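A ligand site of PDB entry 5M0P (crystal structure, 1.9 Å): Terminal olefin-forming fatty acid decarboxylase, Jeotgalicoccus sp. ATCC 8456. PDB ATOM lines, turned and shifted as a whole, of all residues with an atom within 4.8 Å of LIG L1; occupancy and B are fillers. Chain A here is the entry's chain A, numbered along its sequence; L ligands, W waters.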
ATOM      1  N   TYR A  65      13.448  32.184 -14.033  1.00  0.00           N
ATOM      2  CA  TYR A  65      14.201  31.283 -14.838  1.00  0.00           C
ATOM      3  C   TYR A  65      14.242  31.669 -16.300  1.00  0.00           C
ATOM      4  O   TYR A  65      14.670  30.887 -17.138  1.00  0.00           O
ATOM      5  CB  TYR A  65      13.698  29.839 -14.666  1.00  0.00           C
ATOM      6  CG  TYR A  65      14.134  29.243 -13.354  1.00  0.00           C
ATOM      7  CD1 TYR A  65      15.467  28.856 -13.135  1.00  0.00           C
ATOM      8  CD2 TYR A  65      13.227  29.054 -12.318  1.00  0.00           C
ATOM      9  CE1 TYR A  65      15.865  28.341 -11.916  1.00  0.00           C
ATOM     10  CE2 TYR A  65      13.611  28.490 -11.104  1.00  0.00           C
ATOM     11  CZ  TYR A  65      14.949  28.143 -10.898  1.00  0.00           C
ATOM     12  OH  TYR A  65      15.328  27.595  -9.717  1.00  0.00           O
ATOM     13  N   ARG A  72      22.204  34.844 -12.841  1.00  0.00           N
ATOM     14  CA  ARG A  72      22.552  34.119 -11.608  1.00  0.00           C
ATOM     15  C   ARG A  72      24.020  34.296 -11.224  1.00  0.00           C
ATOM     16  O   ARG A  72      24.389  34.048 -10.079  1.00  0.00           O
ATOM     17  CB  ARG A  72      22.211  32.643 -11.758  1.00  0.00           C
ATOM     18  CG  ARG A  72      20.769  32.385 -12.145  1.00  0.00           C
ATOM     19  CD  ARG A  72      19.750  32.810 -11.055  1.00  0.00           C
ATOM     20  NE  ARG A  72      19.958  32.139  -9.789  1.00  0.00           N
ATOM     21  CZ  ARG A  72      19.588  30.882  -9.526  1.00  0.00           C
ATOM     22  NH1 ARG A  72      18.949  30.146 -10.420  1.00  0.00           N
ATOM     23  NH2 ARG A  72      19.857  30.355  -8.338  1.00  0.00           N
ATOM     24  N   ILE A  90      29.552  24.319 -10.702  1.00  0.00           N
ATOM     25  CA  ILE A  90      28.515  24.486 -11.701  1.00  0.00           C
ATOM     26  C   ILE A  90      27.527  25.587 -11.308  1.00  0.00           C
ATOM     27  O   ILE A  90      26.982  26.263 -12.172  1.00  0.00           O
ATOM     28  CB  ILE A  90      27.778  23.134 -11.917  1.00  0.00           C
ATOM     29  CG1 ILE A  90      26.627  23.267 -12.921  1.00  0.00           C
ATOM     30  CG2 ILE A  90      27.268  22.579 -10.614  1.00  0.00           C
ATOM     31  CD1 ILE A  90      27.073  23.207 -14.341  1.00  0.00           C
ATOM     32  N   HIS A  91      27.285  25.777 -10.011  1.00  0.00           N
ATOM     33  CA  HIS A  91      26.319  26.780  -9.548  1.00  0.00           C
ATOM     34  C   HIS A  91      26.780  28.200  -9.915  1.00  0.00           C
ATOM     35  O   HIS A  91      25.967  29.079 -10.067  1.00  0.00           O
ATOM     36  CB  HIS A  91      26.139  26.726  -8.032  1.00  0.00           C
ATOM     37  CG  HIS A  91      25.841  25.379  -7.494  1.00  0.00           C
ATOM     38  ND1 HIS A  91      26.786  24.374  -7.404  1.00  0.00           N
ATOM     39  CD2 HIS A  91      24.709  24.870  -6.956  1.00  0.00           C
ATOM     40  CE1 HIS A  91      26.235  23.302  -6.877  1.00  0.00           C
ATOM     41  NE2 HIS A  91      24.971  23.585  -6.575  1.00  0.00           N
ATOM     42  N   HIS A  98      27.996  27.014 -18.663  1.00  0.00           N
ATOM     43  CA  HIS A  98      27.086  26.316 -17.751  1.00  0.00           C
ATOM     44  C   HIS A  98      26.308  25.226 -18.488  1.00  0.00           C
ATOM     45  O   HIS A  98      26.178  24.132 -17.999  1.00  0.00           O
ATOM     46  CB  HIS A  98      26.090  27.277 -17.096  1.00  0.00           C
ATOM     47  CG  HIS A  98      25.010  26.577 -16.346  1.00  0.00           C
ATOM     48  ND1 HIS A  98      23.756  26.397 -16.875  1.00  0.00           N
ATOM     49  CD2 HIS A  98      25.009  25.926 -15.166  1.00  0.00           C
ATOM     50  CE1 HIS A  98      23.015  25.710 -16.037  1.00  0.00           C
ATOM     51  NE2 HIS A  98      23.757  25.408 -14.993  1.00  0.00           N
ATOM     52  N   LYS A 102      26.441  21.493 -17.398  1.00  0.00           N
ATOM     53  CA  LYS A 102      25.192  20.903 -16.910  1.00  0.00           C
ATOM     54  C   LYS A 102      24.815  19.629 -17.670  1.00  0.00           C
ATOM     55  O   LYS A 102      24.244  18.713 -17.089  1.00  0.00           O
ATOM     56  CB  LYS A 102      24.073  21.919 -16.992  1.00  0.00           C
ATOM     57  CG  LYS A 102      22.763  21.465 -16.384  1.00  0.00           C
ATOM     58  CD  LYS A 102      22.908  20.999 -14.950  1.00  0.00           C
ATOM     59  CE  LYS A 102      21.582  20.861 -14.254  1.00  0.00           C
ATOM     60  NZ  LYS A 102      20.829  22.119 -14.112  1.00  0.00           N
ATOM     61  N   PHE A 105      26.446  16.735 -15.950  1.00  0.00           N
ATOM     62  CA  PHE A 105      25.673  16.318 -14.759  1.00  0.00           C
ATOM     63  C   PHE A 105      24.457  15.513 -15.144  1.00  0.00           C
ATOM     64  O   PHE A 105      24.203  14.430 -14.566  1.00  0.00           O
ATOM     65  CB  PHE A 105      25.251  17.509 -13.894  1.00  0.00           C
ATOM     66  CG  PHE A 105      26.341  18.026 -13.006  1.00  0.00           C
ATOM     67  CD1 PHE A 105      27.264  18.945 -13.462  1.00  0.00           C
ATOM     68  CD2 PHE A 105      26.408  17.621 -11.688  1.00  0.00           C
ATOM     69  CE1 PHE A 105      28.265  19.424 -12.636  1.00  0.00           C
ATOM     70  CE2 PHE A 105      27.388  18.113 -10.847  1.00  0.00           C
ATOM     71  CZ  PHE A 105      28.323  18.987 -11.329  1.00  0.00           C
ATOM     72  N   MET A 109      22.172  10.755 -15.222  1.00  0.00           N
ATOM     73  CA  MET A 109      20.827  10.392 -14.747  1.00  0.00           C
ATOM     74  C   MET A 109      20.135   9.464 -15.738  1.00  0.00           C
ATOM     75  O   MET A 109      19.018   9.701 -16.164  1.00  0.00           O
ATOM     76  CB  MET A 109      20.001  11.659 -14.526  1.00  0.00           C
ATOM     77  CG  MET A 109      20.698  12.687 -13.648  1.00  0.00           C
ATOM     78  SD  MET A 109      21.277  11.918 -12.109  1.00  0.00           S
ATOM     79  CE  MET A 109      22.226  13.282 -11.382  1.00  0.00           C
ATOM     80  N   TRP A 155      27.610   5.200  -5.573  1.00  0.00           N
ATOM     81  CA  TRP A 155      26.941   5.576  -6.804  1.00  0.00           C
ATOM     82  C   TRP A 155      27.831   6.482  -7.662  1.00  0.00           C
ATOM     83  O   TRP A 155      27.814   6.388  -8.885  1.00  0.00           O
ATOM     84  CB  TRP A 155      25.596   6.287  -6.502  1.00  0.00           C
ATOM     85  CG  TRP A 155      24.892   6.712  -7.741  1.00  0.00           C
ATOM     86  CD1 TRP A 155      24.132   5.928  -8.522  1.00  0.00           C
ATOM     87  CD2 TRP A 155      24.882   8.009  -8.348  1.00  0.00           C
ATOM     88  NE1 TRP A 155      23.644   6.639  -9.588  1.00  0.00           N
ATOM     89  CE2 TRP A 155      24.112   7.920  -9.516  1.00  0.00           C
ATOM     90  CE3 TRP A 155      25.454   9.232  -8.023  1.00  0.00           C
ATOM     91  CZ2 TRP A 155      23.902   8.986 -10.345  1.00  0.00           C
ATOM     92  CZ3 TRP A 155      25.239  10.319  -8.849  1.00  0.00           C
ATOM     93  CH2 TRP A 155      24.467  10.179 -10.017  1.00  0.00           C
ATOM     94  N   ASN A 248      29.656  17.825  -6.062  1.00  0.00           N
ATOM     95  CA  ASN A 248      28.315  18.261  -6.332  1.00  0.00           C
ATOM     96  C   ASN A 248      27.415  17.168  -6.835  1.00  0.00           C
ATOM     97  O   ASN A 248      26.205  17.380  -6.995  1.00  0.00           O
ATOM     98  CB  ASN A 248      28.309  19.486  -7.255  1.00  0.00           C
ATOM     99  CG  ASN A 248      28.847  20.745  -6.545  1.00  0.00           C
ATOM    100  OD1 ASN A 248      28.714  20.900  -5.349  1.00  0.00           O
ATOM    101  ND2 ASN A 248      29.465  21.620  -7.281  1.00  0.00           N
ATOM    102  N   THR A 249      27.979  16.001  -7.186  1.00  0.00           N
ATOM    103  CA  THR A 249      27.188  14.897  -7.639  1.00  0.00           C
ATOM    104  C   THR A 249      26.663  14.000  -6.524  1.00  0.00           C
ATOM    105  O   THR A 249      25.765  13.183  -6.802  1.00  0.00           O
ATOM    106  CB  THR A 249      27.918  13.975  -8.629  1.00  0.00           C
ATOM    107  OG1 THR A 249      28.939  13.233  -7.942  1.00  0.00           O
ATOM    108  CG2 THR A 249      28.492  14.790  -9.782  1.00  0.00           C
ATOM    109  N   PRO A 252      24.866  16.493  -2.210  1.00  0.00           N
ATOM    110  CA  PRO A 252      23.439  16.720  -2.055  1.00  0.00           C
ATOM    111  C   PRO A 252      22.630  15.426  -1.967  1.00  0.00           C
ATOM    112  O   PRO A 252      21.550  15.437  -1.393  1.00  0.00           O
ATOM    113  CB  PRO A 252      23.072  17.532  -3.280  1.00  0.00           C
ATOM    114  CG  PRO A 252      24.351  18.020  -3.840  1.00  0.00           C
ATOM    115  CD  PRO A 252      25.344  17.016  -3.489  1.00  0.00           C
ATOM    116  N   LEU A 253      23.154  14.323  -2.517  1.00  0.00           N
ATOM    117  CA  LEU A 253      22.533  12.992  -2.266  1.00  0.00           C
ATOM    118  C   LEU A 253      22.586  12.667  -0.782  1.00  0.00           C
ATOM    119  O   LEU A 253      21.592  12.214  -0.212  1.00  0.00           O
ATOM    120  CB  LEU A 253      23.215  11.932  -3.115  1.00  0.00           C
ATOM    121  CG  LEU A 253      22.599  10.535  -3.236  1.00  0.00           C
ATOM    122  CD1 LEU A 253      23.158   9.862  -4.464  1.00  0.00           C
ATOM    123  CD2 LEU A 253      22.871   9.702  -2.017  1.00  0.00           C
ATOM    124  N   ALA A 255      22.596  14.875   1.495  1.00  0.00           N
ATOM    125  CA  ALA A 255      21.691  15.809   2.110  1.00  0.00           C
ATOM    126  C   ALA A 255      20.242  15.311   2.135  1.00  0.00           C
ATOM    127  O   ALA A 255      19.422  15.874   2.853  1.00  0.00           O
ATOM    128  CB  ALA A 255      21.752  17.192   1.396  1.00  0.00           C
ATOM    129  N   ILE A 256      19.917  14.261   1.365  1.00  0.00           N
ATOM    130  CA  ILE A 256      18.620  13.669   1.434  1.00  0.00           C
ATOM    131  C   ILE A 256      18.281  13.220   2.851  1.00  0.00           C
ATOM    132  O   ILE A 256      17.106  13.044   3.162  1.00  0.00           O
ATOM    133  CB  ILE A 256      18.461  12.537   0.401  1.00  0.00           C
ATOM    134  CG1 ILE A 256      18.638  13.093  -1.017  1.00  0.00           C
ATOM    135  CG2 ILE A 256      17.081  11.892   0.442  1.00  0.00           C
ATOM    136  CD1 ILE A 256      18.689  12.021  -2.094  1.00  0.00           C
ATOM    137  N   PHE A 259      15.461  15.051   4.273  1.00  0.00           N
ATOM    138  CA  PHE A 259      14.132  14.610   3.859  1.00  0.00           C
ATOM    139  C   PHE A 259      13.734  13.262   4.462  1.00  0.00           C
ATOM    140  O   PHE A 259      12.551  12.998   4.651  1.00  0.00           O
ATOM    141  CB  PHE A 259      14.026  14.516   2.346  1.00  0.00           C
ATOM    142  CG  PHE A 259      13.883  15.852   1.648  1.00  0.00           C
ATOM    143  CD1 PHE A 259      13.068  16.824   2.166  1.00  0.00           C
ATOM    144  CD2 PHE A 259      14.495  16.080   0.409  1.00  0.00           C
ATOM    145  CE1 PHE A 259      12.882  18.022   1.511  1.00  0.00           C
ATOM    146  CE2 PHE A 259      14.312  17.266  -0.258  1.00  0.00           C
ATOM    147  CZ  PHE A 259      13.524  18.253   0.311  1.00  0.00           C
ATOM    148  N   PHE A 297      13.239  23.494   3.346  1.00  0.00           N
ATOM    149  CA  PHE A 297      14.634  23.199   3.150  1.00  0.00           C
ATOM    150  C   PHE A 297      15.311  24.423   2.523  1.00  0.00           C
ATOM    151  O   PHE A 297      15.961  25.199   3.215  1.00  0.00           O
ATOM    152  CB  PHE A 297      14.839  21.926   2.300  1.00  0.00           C
ATOM    153  CG  PHE A 297      16.208  21.302   2.433  1.00  0.00           C
ATOM    154  CD1 PHE A 297      17.361  22.065   2.611  1.00  0.00           C
ATOM    155  CD2 PHE A 297      16.345  19.931   2.309  1.00  0.00           C
ATOM    156  CE1 PHE A 297      18.589  21.468   2.703  1.00  0.00           C
ATOM    157  CE2 PHE A 297      17.575  19.322   2.389  1.00  0.00           C
ATOM    158  CZ  PHE A 297      18.706  20.087   2.601  1.00  0.00           C
ATOM    159  N   VAL A 298      15.114  24.612   1.235  1.00  0.00           N
ATOM    160  CA  VAL A 298      15.630  25.806   0.535  1.00  0.00           C
ATOM    161  C   VAL A 298      14.627  26.966   0.740  1.00  0.00           C
ATOM    162  O   VAL A 298      13.458  26.843   0.342  1.00  0.00           O
ATOM    163  CB  VAL A 298      15.829  25.540  -0.956  1.00  0.00           C
ATOM    164  CG1 VAL A 298      16.327  26.782  -1.666  1.00  0.00           C
ATOM    165  CG2 VAL A 298      16.790  24.354  -1.130  1.00  0.00           C
ATOM    166  N   LEU A 301      16.086  31.605  -3.508  1.00  0.00           N
ATOM    167  CA  LEU A 301      17.241  31.547  -4.405  1.00  0.00           C
ATOM    168  C   LEU A 301      17.555  32.971  -4.933  1.00  0.00           C
ATOM    169  O   LEU A 301      16.650  33.727  -5.278  1.00  0.00           O
ATOM    170  CB  LEU A 301      16.934  30.594  -5.599  1.00  0.00           C
ATOM    171  CG  LEU A 301      16.852  29.096  -5.199  1.00  0.00           C
ATOM    172  CD1 LEU A 301      16.365  28.244  -6.335  1.00  0.00           C
ATOM    173  CD2 LEU A 301      18.180  28.595  -4.734  1.00  0.00           C
ATOM    174  N   PRO A 359      10.825  22.865  -4.792  1.00  0.00           N
ATOM    175  CA  PRO A 359      11.690  22.811  -3.629  1.00  0.00           C
ATOM    176  C   PRO A 359      13.172  22.608  -3.967  1.00  0.00           C
ATOM    177  O   PRO A 359      14.039  22.853  -3.127  1.00  0.00           O
ATOM    178  CB  PRO A 359      11.136  21.614  -2.846  1.00  0.00           C
ATOM    179  CG  PRO A 359      10.623  20.737  -3.864  1.00  0.00           C
ATOM    180  CD  PRO A 359       9.989  21.647  -4.894  1.00  0.00           C
ATOM    181  N   GLN A 360      13.469  22.169  -5.184  1.00  0.00           N
ATOM    182  CA  GLN A 360      14.842  22.025  -5.677  1.00  0.00           C
ATOM    183  C   GLN A 360      15.013  22.807  -6.975  1.00  0.00           C
ATOM    184  O   GLN A 360      15.736  22.408  -7.866  1.00  0.00           O
ATOM    185  CB  GLN A 360      15.170  20.522  -5.859  1.00  0.00           C
ATOM    186  CG  GLN A 360      14.966  19.755  -4.551  1.00  0.00           C
ATOM    187  CD  GLN A 360      15.167  18.259  -4.658  1.00  0.00           C
ATOM    188  OE1 GLN A 360      14.348  17.500  -4.143  1.00  0.00           O
ATOM    189  NE2 GLN A 360      16.283  17.815  -5.289  1.00  0.00           N
ATOM    190  N   GLY A 361      14.335  23.933  -7.070  1.00  0.00           N
ATOM    191  CA  GLY A 361      14.421  24.755  -8.198  1.00  0.00           C
ATOM    192  C   GLY A 361      13.325  24.528  -9.201  1.00  0.00           C
ATOM    193  O   GLY A 361      12.574  23.548  -9.137  1.00  0.00           O
ATOM    194  N   ASN A 368      18.619  25.834 -17.281  1.00  0.00           N
ATOM    195  CA  ASN A 368      18.547  26.555 -16.035  1.00  0.00           C
ATOM    196  C   ASN A 368      19.410  25.869 -14.974  1.00  0.00           C
ATOM    197  O   ASN A 368      19.902  24.770 -15.189  1.00  0.00           O
ATOM    198  CB  ASN A 368      17.123  26.672 -15.562  1.00  0.00           C
ATOM    199  CG  ASN A 368      16.275  27.614 -16.418  1.00  0.00           C
ATOM    200  OD1 ASN A 368      15.231  27.224 -16.954  1.00  0.00           O
ATOM    201  ND2 ASN A 368      16.733  28.842 -16.553  1.00  0.00           N
ATOM    202  N   HIS A 369      19.570  26.532 -13.830  1.00  0.00           N
ATOM    203  CA  HIS A 369      20.281  26.008 -12.698  1.00  0.00           C
ATOM    204  C   HIS A 369      19.480  25.003 -11.850  1.00  0.00           C
ATOM    205  O   HIS A 369      19.896  24.669 -10.756  1.00  0.00           O
ATOM    206  CB  HIS A 369      20.793  27.144 -11.855  1.00  0.00           C
ATOM    207  CG  HIS A 369      21.993  27.823 -12.427  1.00  0.00           C
ATOM    208  ND1 HIS A 369      23.279  27.365 -12.200  1.00  0.00           N
ATOM    209  CD2 HIS A 369      22.120  28.951 -13.160  1.00  0.00           C
ATOM    210  CE1 HIS A 369      24.146  28.172 -12.784  1.00  0.00           C
ATOM    211  NE2 HIS A 369      23.476  29.153 -13.355  1.00  0.00           N
ATOM    212  N   ARG A 370      18.356  24.533 -12.362  1.00  0.00           N
ATOM    213  CA  ARG A 370      17.507  23.595 -11.660  1.00  0.00           C
ATOM    214  C   ARG A 370      18.301  22.363 -11.202  1.00  0.00           C
ATOM    215  O   ARG A 370      19.211  21.912 -11.866  1.00  0.00           O
ATOM    216  CB  ARG A 370      16.357  23.115 -12.592  1.00  0.00           C
ATOM    217  CG  ARG A 370      15.334  22.262 -11.890  1.00  0.00           C
ATOM    218  CD  ARG A 370      14.230  21.812 -12.840  1.00  0.00           C
ATOM    219  NE  ARG A 370      13.216  21.067 -12.134  1.00  0.00           N
ATOM    220  CZ  ARG A 370      11.945  21.414 -12.015  1.00  0.00           C
ATOM    221  NH1 ARG A 370      11.487  22.529 -12.570  1.00  0.00           N
ATOM    222  NH2 ARG A 370      11.127  20.622 -11.325  1.00  0.00           N
ATOM    223  N   CYS A 371      17.940  21.870 -10.030  1.00  0.00           N
ATOM    224  CA  CYS A 371      18.600  20.714  -9.419  1.00  0.00           C
ATOM    225  C   CYS A 371      18.740  19.561 -10.391  1.00  0.00           C
ATOM    226  O   CYS A 371      17.783  19.157 -11.023  1.00  0.00           O
ATOM    227  CB  CYS A 371      17.820  20.254  -8.228  1.00  0.00           C
ATOM    228  SG  CYS A 371      18.526  18.817  -7.391  1.00  0.00           S
ATOM    229  N   ALA A 372      19.953  19.013 -10.475  1.00  0.00           N
ATOM    230  CA  ALA A 372      20.176  17.851 -11.340  1.00  0.00           C
ATOM    231  C   ALA A 372      19.684  16.549 -10.718  1.00  0.00           C
ATOM    232  O   ALA A 372      19.442  15.558 -11.424  1.00  0.00           O
ATOM    233  CB  ALA A 372      21.695  17.741 -11.654  1.00  0.00           C
ATOM    234  N   GLY A 373      19.570  16.526  -9.389  1.00  0.00           N
ATOM    235  CA  GLY A 373      19.317  15.322  -8.632  1.00  0.00           C
ATOM    236  C   GLY A 373      17.907  15.101  -8.150  1.00  0.00           C
ATOM    237  O   GLY A 373      17.702  14.320  -7.229  1.00  0.00           O
ATOM    238  N   ILE A 376      16.818  11.374  -8.371  1.00  0.00           N
ATOM    239  CA  ILE A 376      17.479  10.609  -7.345  1.00  0.00           C
ATOM    240  C   ILE A 376      16.833  10.888  -5.990  1.00  0.00           C
ATOM    241  O   ILE A 376      16.662   9.978  -5.179  1.00  0.00           O
ATOM    242  CB  ILE A 376      19.004  10.905  -7.339  1.00  0.00           C
ATOM    243  CG1 ILE A 376      19.666  10.249  -8.546  1.00  0.00           C
ATOM    244  CG2 ILE A 376      19.641  10.413  -6.067  1.00  0.00           C
ATOM    245  CD1 ILE A 376      21.062  10.737  -8.790  1.00  0.00           C
ATOM    246  N   THR A 377      16.524  12.159  -5.697  1.00  0.00           N
ATOM    247  CA  THR A 377      15.923  12.490  -4.456  1.00  0.00           C
ATOM    248  C   THR A 377      14.605  11.745  -4.225  1.00  0.00           C
ATOM    249  O   THR A 377      14.411  11.131  -3.176  1.00  0.00           O
ATOM    250  CB  THR A 377      15.685  14.036  -4.335  1.00  0.00           C
ATOM    251  OG1 THR A 377      16.919  14.729  -4.505  1.00  0.00           O
ATOM    252  CG2 THR A 377      15.146  14.388  -3.015  1.00  0.00           C
HETATM  253  C1  LIG L   1      21.037  22.680  -7.606  1.00  0.00           C
HETATM  254  C2  LIG L   1      18.131  21.670  -3.908  1.00  0.00           C
HETATM  255  C3  LIG L   1      19.450  17.054  -4.020  1.00  0.00           C
HETATM  256  C4  LIG L   1      22.612  18.085  -7.511  1.00  0.00           C
HETATM  257  C5  LIG L   1      20.067  22.796  -6.642  1.00  0.00           C
HETATM  258  C6  LIG L   1      19.329  24.003  -6.345  1.00  0.00           C
HETATM  259  C7  LIG L   1      18.536  23.727  -5.282  1.00  0.00           C
HETATM  260  C8  LIG L   1      18.741  22.330  -4.939  1.00  0.00           C
HETATM  261  C9  LIG L   1      17.595  24.673  -4.581  1.00  0.00           C
HETATM  262  C10 LIG L   1      19.498  25.360  -7.012  1.00  0.00           C
HETATM  263  C11 LIG L   1      18.453  25.591  -8.126  1.00  0.00           C
HETATM  264  C12 LIG L   1      18.750  26.924  -8.825  1.00  0.00           C
HETATM  265  O1  LIG L   1      17.951  27.447  -9.639  1.00  0.00           O
HETATM  266  O2  LIG L   1      19.818  27.517  -8.542  1.00  0.00           O
HETATM  267  C13 LIG L   1      18.329  20.358  -3.551  1.00  0.00           C
HETATM  268  C14 LIG L   1      17.761  19.754  -2.366  1.00  0.00           C
HETATM  269  C15 LIG L   1      18.101  18.454  -2.355  1.00  0.00           C
HETATM  270  C16 LIG L   1      18.922  18.239  -3.568  1.00  0.00           C
HETATM  271  C17 LIG L   1      16.923  20.467  -1.322  1.00  0.00           C
HETATM  272  C18 LIG L   1      17.752  17.513  -1.231  1.00  0.00           C
HETATM  273  C19 LIG L   1      18.555  16.518  -0.891  1.00  0.00           C
HETATM  274  C20 LIG L   1      20.368  16.880  -5.031  1.00  0.00           C
HETATM  275  C21 LIG L   1      20.985  15.642  -5.439  1.00  0.00           C
HETATM  276  C22 LIG L   1      21.881  15.920  -6.417  1.00  0.00           C
HETATM  277  C23 LIG L   1      21.828  17.351  -6.613  1.00  0.00           C
HETATM  278  C24 LIG L   1      20.566  14.300  -4.856  1.00  0.00           C
HETATM  279  C25 LIG L   1      22.781  15.039  -7.227  1.00  0.00           C
HETATM  280  C26 LIG L   1      22.650  13.684  -7.274  1.00  0.00           C
HETATM  281  C27 LIG L   1      22.451  19.436  -7.797  1.00  0.00           C
HETATM  282  C28 LIG L   1      23.303  20.175  -8.740  1.00  0.00           C
HETATM  283  C29 LIG L   1      22.881  21.436  -8.775  1.00  0.00           C
HETATM  284  C30 LIG L   1      21.749  21.500  -7.855  1.00  0.00           C
HETATM  285  C31 LIG L   1      24.446  19.619  -9.492  1.00  0.00           C
HETATM  286  C32 LIG L   1      23.440  22.617  -9.592  1.00  0.00           C
HETATM  287  C33 LIG L   1      22.767  22.645 -10.950  1.00  0.00           C
HETATM  288  C34 LIG L   1      23.099  23.902 -11.738  1.00  0.00           C
HETATM  289  O3  LIG L   1      22.796  23.910 -12.966  1.00  0.00           O
HETATM  290  O4  LIG L   1      23.643  24.867 -11.173  1.00  0.00           O
HETATM  291  N1  LIG L   1      19.640  21.789  -5.806  1.00  0.00           N
HETATM  292  N2  LIG L   1      18.984  19.416  -4.243  1.00  0.00           N
HETATM  293  N3  LIG L   1      20.906  17.871  -5.772  1.00  0.00           N
HETATM  294  N4  LIG L   1      21.505  20.246  -7.294  1.00  0.00           N
HETATM  295 FE1  LIG L   1      20.237  19.823  -5.825  1.00  0.00          FE
HETATM  296  O1  LG2 L   2      23.975  21.313  -2.325  1.00  0.00           O
HETATM  297  C1  LG2 L   2      23.585  20.633  -1.339  1.00  0.00           C
HETATM  298  O2  LG2 L   2      24.419  20.237  -0.518  1.00  0.00           O
HETATM  299  C2  LG2 L   2      22.094  20.237  -1.179  1.00  0.00           C
HETATM  300  C3  LG2 L   2      21.401  21.146  -0.207  1.00  0.00           C
HETATM  301  C4  LG2 L   2      20.524  22.107  -0.973  1.00  0.00           C
HETATM  302  C5  LG2 L   2      21.221  23.469  -1.135  1.00  0.00           C
HETATM  303  C6  LG2 L   2      20.530  24.543  -0.311  1.00  0.00           C
HETATM  304  C7  LG2 L   2      20.729  25.905  -1.008  1.00  0.00           C
HETATM  305  C8  LG2 L   2      20.355  27.045  -0.062  1.00  0.00           C
HETATM  306  C9  LG2 L   2      20.758  28.355  -0.692  1.00  0.00           C
HETATM  307  C10 LG2 L   2      20.407  29.524   0.180  1.00  0.00           C
HETATM  308  C11 LG2 L   2      20.492  30.770  -0.640  1.00  0.00           C
HETATM  309  C12 LG2 L   2      20.561  32.010   0.235  1.00  0.00           C
HETATM  310  C13 LG2 L   2      20.594  33.243  -0.668  1.00  0.00           C
HETATM  311  C14 LG2 L   2      20.611  34.531   0.112  1.00  0.00           C
HETATM  312  C15 LG2 L   2      19.677  35.539  -0.559  1.00  0.00           C
HETATM  313  C16 LG2 L   2      19.201  36.576   0.452  1.00  0.00           C
HETATM  314  C17 LG2 L   2      17.972  37.313  -0.087  1.00  0.00           C
HETATM  315  C18 LG2 L   2      16.977  37.598   1.033  1.00  0.00           C
HETATM  316  C19 LG2 L   2      15.587  37.339   0.479  1.00  0.00           C
HETATM  317  C20 LG2 L   2      14.556  37.734   1.513  1.00  0.00           C
HETATM  318  O   HOH W   1      22.603  26.787  -8.613  1.00  0.00           O
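A nitrogen (N2) of LIG L1 lies close to the side-chain amide nitrogen of Gln 360 (3.3 Å). Ile 90 touches LIG L1 (O to O4, 3.8 Å). NE2 of His 91 touches C32 of LIG L1, at 3.5 Å. CD2 of Phe 105 touches C31 of LIG L1 (3.6 Å). Asn 248 touches LIG L1 (O to C4, 3.7 Å). Thr 249 touches LIG L1. Pro 252 touches LIG L1. Leu 253 touches LIG L1. C of Ala 255 touches C19 of LIG L1, 3.7 Å away. Ile 256 touches LIG L1 (CG1 to C19, 3.4 Å). Phe 259 touches LIG L1 (CE2 to C18, 3.6 Å). CD2 of Phe 297 touches C17 of LIG L1 (3.7 Å). Val 298 touches LIG L1 (CG2 to C9, 3.6 Å). Leu 301 touches LIG L1. O of Asn 368 touches O3 of LIG L1 (3.7 Å). O of Arg 370 touches C33 of LIG L1 (3.7 Å). Ala 372 touches LIG L1. Gly 373 touches LIG L1 (CA to C22, 3.4 Å). Ile 376 touches LIG L1 (CD1 to C26, 3.7 Å). Thr 377 touches LIG L1 (OG1 to C3, 3.5 Å). Hydrophobic or aromatic side chains within 4 Å of LIG L1: Tyr 65, Ile 90, His 91, His 98, Phe 105, Pro 252, Leu 253, Ala 255, Ile 256, Phe 259, Phe 297, Val 298, Leu 301, His 369, Ala 372 and Ile 376. Within 4 Å of LIG L1: Tyr 65, Arg 72, Ile 90, His 91, His 98, Lys 102, Phe 105, Asn 248, Thr 249, Pro 252, Leu 253, Ala 255, Ile 256, Phe 259, Phe 297, Val 298, Leu 301, Gln 360, Asn 368, His 369, Arg 370, Cys 371, Ala 372, Gly 373, Ile 376 and Thr 377. The nearest printed residue that does not touch LIG L1 is Gly 361 (4.1 Å).
The backbone carbonyl oxygen (O) of Gln 360 sits close to the backbone NH (N) of Cys 371. SG of Cys 371 lies close to N of Gly 373 (3.2 Å). The backbone carbonyl oxygen (O) of Tyr 65 lies within hydrogen-bond range of the side-chain amide nitrogen (ND2) of Asn 368, 3.0 Å away. A ring nitrogen (NE2) of His 98 is in hydrogen-bond range of a ring nitrogen (ND1) of His 369 (3.4 Å). The side-chain amino group of Lys 102 lies within hydrogen-bond range of the backbone carbonyl oxygen of Arg 370, at 2.8 Å. NZ of Lys 102 is in hydrogen-bond range of O of Asn 368 (3.0 Å). NE2 of Gln 360 sits at hydrogen-bond distance from OG1 of Thr 377 (3.2 Å). The side-chain hydroxyl (OG1) of Thr 377 is in hydrogen-bond range of the backbone carbonyl oxygen (O) of Gly 373, at 2.9 Å.
An iron atom (FE1) of LIG L1 is bound by the side-chain sulfur (SG) of Cys 371 (2.5 Å). The side-chain hydroxyl (OH) of Tyr 65 lies within hydrogen-bond range of an oxygen (O1) of LIG L1 (2.6 Å). An oxygen (O3) of LIG L1 is in hydrogen-bond range of a ring nitrogen (NE2) of His 98, at 2.7 Å. A ring nitrogen (ND1) of His 369 is in hydrogen-bond range of an oxygen (O4) of LIG L1. O2 of LIG L1 is in salt-bridge range of NH2 of Arg 72 (2.8 Å). NZ of Lys 102 is in salt-bridge range of O3 of LIG L1 (2.9 Å).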
